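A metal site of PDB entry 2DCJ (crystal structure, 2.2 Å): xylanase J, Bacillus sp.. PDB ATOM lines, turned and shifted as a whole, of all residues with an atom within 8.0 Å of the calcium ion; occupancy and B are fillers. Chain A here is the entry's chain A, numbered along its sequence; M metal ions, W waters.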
ATOM      1  N   TYR A 250     -26.958   1.070 -28.369  1.00  0.00           N
ATOM      2  CA  TYR A 250     -26.407   0.512 -29.620  1.00  0.00           C
ATOM      3  C   TYR A 250     -25.287  -0.453 -29.483  1.00  0.00           C
ATOM      4  O   TYR A 250     -24.798  -0.998 -30.494  1.00  0.00           O
ATOM      5  CB  TYR A 250     -25.916   1.698 -30.537  1.00  0.00           C
ATOM      6  CG  TYR A 250     -26.968   2.757 -30.807  1.00  0.00           C
ATOM      7  CD1 TYR A 250     -28.060   2.499 -31.640  1.00  0.00           C
ATOM      8  CD2 TYR A 250     -26.891   3.982 -30.244  1.00  0.00           C
ATOM      9  CE1 TYR A 250     -29.056   3.485 -31.890  1.00  0.00           C
ATOM     10  CE2 TYR A 250     -27.864   4.954 -30.456  1.00  0.00           C
ATOM     11  CZ  TYR A 250     -28.928   4.693 -31.291  1.00  0.00           C
ATOM     12  OH  TYR A 250     -29.857   5.664 -31.482  1.00  0.00           O
ATOM     13  N   LEU A 263     -18.888   0.893 -28.517  1.00  0.00           N
ATOM     14  CA  LEU A 263     -19.806   1.702 -27.786  1.00  0.00           C
ATOM     15  C   LEU A 263     -19.960   3.044 -28.584  1.00  0.00           C
ATOM     16  O   LEU A 263     -18.939   3.744 -28.795  1.00  0.00           O
ATOM     17  CB  LEU A 263     -19.267   1.986 -26.367  1.00  0.00           C
ATOM     18  CG  LEU A 263     -18.675   0.790 -25.568  1.00  0.00           C
ATOM     19  CD1 LEU A 263     -18.160   1.258 -24.226  1.00  0.00           C
ATOM     20  CD2 LEU A 263     -19.815  -0.300 -25.374  1.00  0.00           C
ATOM     21  N   TYR A 264     -21.206   3.415 -28.904  1.00  0.00           N
ATOM     22  CA  TYR A 264     -21.510   4.444 -29.904  1.00  0.00           C
ATOM     23  C   TYR A 264     -22.111   5.649 -29.309  1.00  0.00           C
ATOM     24  O   TYR A 264     -21.941   6.706 -29.872  1.00  0.00           O
ATOM     25  CB  TYR A 264     -22.504   3.926 -30.952  1.00  0.00           C
ATOM     26  CG  TYR A 264     -22.042   2.756 -31.781  1.00  0.00           C
ATOM     27  CD1 TYR A 264     -21.303   2.940 -32.948  1.00  0.00           C
ATOM     28  CD2 TYR A 264     -22.370   1.445 -31.421  1.00  0.00           C
ATOM     29  CE1 TYR A 264     -20.867   1.838 -33.740  1.00  0.00           C
ATOM     30  CE2 TYR A 264     -21.961   0.343 -32.195  1.00  0.00           C
ATOM     31  CZ  TYR A 264     -21.249   0.538 -33.352  1.00  0.00           C
ATOM     32  OH  TYR A 264     -20.847  -0.528 -34.090  1.00  0.00           O
ATOM     33  N   ALA A 265     -22.929   5.514 -28.248  1.00  0.00           N
ATOM     34  CA  ALA A 265     -23.686   6.642 -27.719  1.00  0.00           C
ATOM     35  C   ALA A 265     -23.634   6.633 -26.220  1.00  0.00           C
ATOM     36  O   ALA A 265     -23.182   5.687 -25.640  1.00  0.00           O
ATOM     37  CB  ALA A 265     -25.107   6.594 -28.189  1.00  0.00           C
ATOM     38  N   ASN A 266     -23.976   7.728 -25.621  1.00  0.00           N
ATOM     39  CA  ASN A 266     -23.899   7.835 -24.184  1.00  0.00           C
ATOM     40  C   ASN A 266     -24.830   6.775 -23.577  1.00  0.00           C
ATOM     41  O   ASN A 266     -25.965   6.613 -24.045  1.00  0.00           O
ATOM     42  CB  ASN A 266     -24.334   9.208 -23.772  1.00  0.00           C
ATOM     43  CG  ASN A 266     -23.262  10.233 -24.015  1.00  0.00           C
ATOM     44  OD1 ASN A 266     -22.075   9.914 -24.047  1.00  0.00           O
ATOM     45  ND2 ASN A 266     -23.674  11.495 -24.135  1.00  0.00           N
ATOM     46  N   ASP A 268     -24.067   3.568 -23.646  1.00  0.00           N
ATOM     47  CA  ASP A 268     -23.520   2.338 -24.149  1.00  0.00           C
ATOM     48  C   ASP A 268     -22.414   1.894 -23.207  1.00  0.00           C
ATOM     49  O   ASP A 268     -21.513   2.695 -22.803  1.00  0.00           O
ATOM     50  CB  ASP A 268     -22.953   2.479 -25.580  1.00  0.00           C
ATOM     51  CG  ASP A 268     -24.030   2.367 -26.687  1.00  0.00           C
ATOM     52  OD1 ASP A 268     -25.212   2.123 -26.287  1.00  0.00           O
ATOM     53  OD2 ASP A 268     -23.732   2.440 -27.961  1.00  0.00           O
ATOM     54  N   ASN A 290     -12.597   4.941 -33.079  1.00  0.00           N
ATOM     55  CA  ASN A 290     -12.798   4.631 -34.505  1.00  0.00           C
ATOM     56  C   ASN A 290     -12.013   5.562 -35.481  1.00  0.00           C
ATOM     57  O   ASN A 290     -11.905   5.265 -36.667  1.00  0.00           O
ATOM     58  CB  ASN A 290     -14.256   4.667 -34.924  1.00  0.00           C
ATOM     59  CG  ASN A 290     -14.839   6.060 -34.971  1.00  0.00           C
ATOM     60  OD1 ASN A 290     -15.569   6.451 -35.944  1.00  0.00           O
ATOM     61  ND2 ASN A 290     -14.606   6.802 -33.962  1.00  0.00           N
ATOM     62  N   VAL A 337     -19.544   4.723 -21.976  1.00  0.00           N
ATOM     63  CA  VAL A 337     -19.419   6.005 -22.667  1.00  0.00           C
ATOM     64  C   VAL A 337     -20.397   7.003 -22.112  1.00  0.00           C
ATOM     65  O   VAL A 337     -21.556   6.747 -22.114  1.00  0.00           O
ATOM     66  CB  VAL A 337     -19.593   5.797 -24.200  1.00  0.00           C
ATOM     67  CG1 VAL A 337     -19.872   7.128 -24.936  1.00  0.00           C
ATOM     68  CG2 VAL A 337     -18.357   5.169 -24.771  1.00  0.00           C
ATOM     69  N   ALA A 339     -19.383  10.675 -22.687  1.00  0.00           N
ATOM     70  CA  ALA A 339     -19.036  11.979 -23.284  1.00  0.00           C
ATOM     71  C   ALA A 339     -19.117  11.953 -24.829  1.00  0.00           C
ATOM     72  O   ALA A 339     -18.395  12.685 -25.527  1.00  0.00           O
ATOM     73  CB  ALA A 339     -17.676  12.418 -22.835  1.00  0.00           C
ATOM     74  N   ASP A 340     -19.948  11.102 -25.381  1.00  0.00           N
ATOM     75  CA  ASP A 340     -20.077  11.035 -26.820  1.00  0.00           C
ATOM     76  C   ASP A 340     -20.767  12.336 -27.338  1.00  0.00           C
ATOM     77  O   ASP A 340     -21.649  12.881 -26.650  1.00  0.00           O
ATOM     78  CB  ASP A 340     -20.883   9.846 -27.228  1.00  0.00           C
ATOM     79  CG  ASP A 340     -21.380   9.930 -28.677  1.00  0.00           C
ATOM     80  OD1 ASP A 340     -20.589   9.707 -29.608  1.00  0.00           O
ATOM     81  OD2 ASP A 340     -22.588   9.976 -29.010  1.00  0.00           O
ATOM     82  N   ASP A 341     -20.364  12.820 -28.524  1.00  0.00           N
ATOM     83  CA  ASP A 341     -21.105  13.895 -29.192  1.00  0.00           C
ATOM     84  C   ASP A 341     -21.261  13.652 -30.708  1.00  0.00           C
ATOM     85  O   ASP A 341     -21.338  14.610 -31.496  1.00  0.00           O
ATOM     86  CB  ASP A 341     -20.426  15.215 -28.890  1.00  0.00           C
ATOM     87  CG  ASP A 341     -19.004  15.271 -29.405  1.00  0.00           C
ATOM     88  OD1 ASP A 341     -18.317  16.256 -29.128  1.00  0.00           O
ATOM     89  OD2 ASP A 341     -18.498  14.399 -30.111  1.00  0.00           O
ATOM     90  N   GLY A 342     -21.246  12.397 -31.117  1.00  0.00           N
ATOM     91  CA  GLY A 342     -21.212  12.061 -32.505  1.00  0.00           C
ATOM     92  C   GLY A 342     -19.909  12.211 -33.274  1.00  0.00           C
ATOM     93  O   GLY A 342     -19.923  11.953 -34.447  1.00  0.00           O
ATOM     94  N   THR A 343     -18.771  12.489 -32.638  1.00  0.00           N
ATOM     95  CA  THR A 343     -17.515  12.579 -33.369  1.00  0.00           C
ATOM     96  C   THR A 343     -16.552  11.409 -33.285  1.00  0.00           C
ATOM     97  O   THR A 343     -15.507  11.426 -33.932  1.00  0.00           O
ATOM     98  CB  THR A 343     -16.784  13.873 -32.980  1.00  0.00           C
ATOM     99  OG1 THR A 343     -16.475  13.891 -31.540  1.00  0.00           O
ATOM    100  CG2 THR A 343     -17.699  15.109 -33.335  1.00  0.00           C
ATOM    101  N   TRP A 344     -16.896  10.391 -32.503  1.00  0.00           N
ATOM    102  CA  TRP A 344     -16.097   9.196 -32.364  1.00  0.00           C
ATOM    103  C   TRP A 344     -16.965   8.106 -31.712  1.00  0.00           C
ATOM    104  O   TRP A 344     -17.891   8.445 -30.984  1.00  0.00           O
ATOM    105  CB  TRP A 344     -14.891   9.428 -31.470  1.00  0.00           C
ATOM    106  CG  TRP A 344     -15.186  10.067 -30.162  1.00  0.00           C
ATOM    107  CD1 TRP A 344     -15.135  11.399 -29.884  1.00  0.00           C
ATOM    108  CD2 TRP A 344     -15.560   9.423 -28.894  1.00  0.00           C
ATOM    109  NE1 TRP A 344     -15.492  11.645 -28.574  1.00  0.00           N
ATOM    110  CE2 TRP A 344     -15.782  10.446 -27.949  1.00  0.00           C
ATOM    111  CE3 TRP A 344     -15.773   8.100 -28.500  1.00  0.00           C
ATOM    112  CZ2 TRP A 344     -16.148  10.191 -26.611  1.00  0.00           C
ATOM    113  CZ3 TRP A 344     -16.170   7.837 -27.192  1.00  0.00           C
ATOM    114  CH2 TRP A 344     -16.376   8.885 -26.261  1.00  0.00           C
ATOM    115  N   ASP A 345     -16.525   6.871 -31.865  1.00  0.00           N
ATOM    116  CA  ASP A 345     -16.993   5.699 -31.163  1.00  0.00           C
ATOM    117  C   ASP A 345     -15.810   5.067 -30.447  1.00  0.00           C
ATOM    118  O   ASP A 345     -14.689   5.287 -30.854  1.00  0.00           O
ATOM    119  CB  ASP A 345     -17.492   4.714 -32.182  1.00  0.00           C
ATOM    120  CG  ASP A 345     -18.650   5.241 -32.983  1.00  0.00           C
ATOM    121  OD1 ASP A 345     -18.776   4.838 -34.177  1.00  0.00           O
ATOM    122  OD2 ASP A 345     -19.517   6.009 -32.491  1.00  0.00           O
ATOM    123  N   ALA A 346     -16.065   4.281 -29.385  1.00  0.00           N
ATOM    124  CA  ALA A 346     -15.021   3.548 -28.657  1.00  0.00           C
ATOM    125  C   ALA A 346     -15.074   2.067 -29.015  1.00  0.00           C
ATOM    126  O   ALA A 346     -16.129   1.462 -28.961  1.00  0.00           O
ATOM    127  CB  ALA A 346     -15.205   3.740 -27.100  1.00  0.00           C
HETATM  128 CA    CA M   1     -20.127   7.774 -30.762  1.00  0.00          CA
HETATM  129  O   HOH W   1     -19.057   6.768 -28.552  1.00  0.00           O
HETATM  130  O   HOH W   2     -21.424   8.585 -33.021  1.00  0.00           O
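The backbone NH of Tyr 264 sits at hydrogen-bond distance from the side-chain carboxylate of Asp 268 (2.9 Å).
N of Gly 342 lies close to OD2 of Asp 340, at 3.5 Å.
The backbone NH (N) of Asp 340 is in hydrogen-bond range of the side-chain amide oxygen (OD1) of Asn 266 (2.8 Å).
N of Asp 345 sits close to ND2 of Asn 290, at 2.8 Å.
Of the 16 residues printed, 4 come within 4 Å of the calcium ion.
The calcium ion is bound by O of Tyr 264 (2.3 Å), OD1 of Asp 340 (2.3 Å), O of Trp 344 (2.3 Å), OD2 of Asp 345 (2.5 Å), water W1 (2.7 Å) and water W2 (2.7 Å).
The calcium ion has six donor atoms within binding distance.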
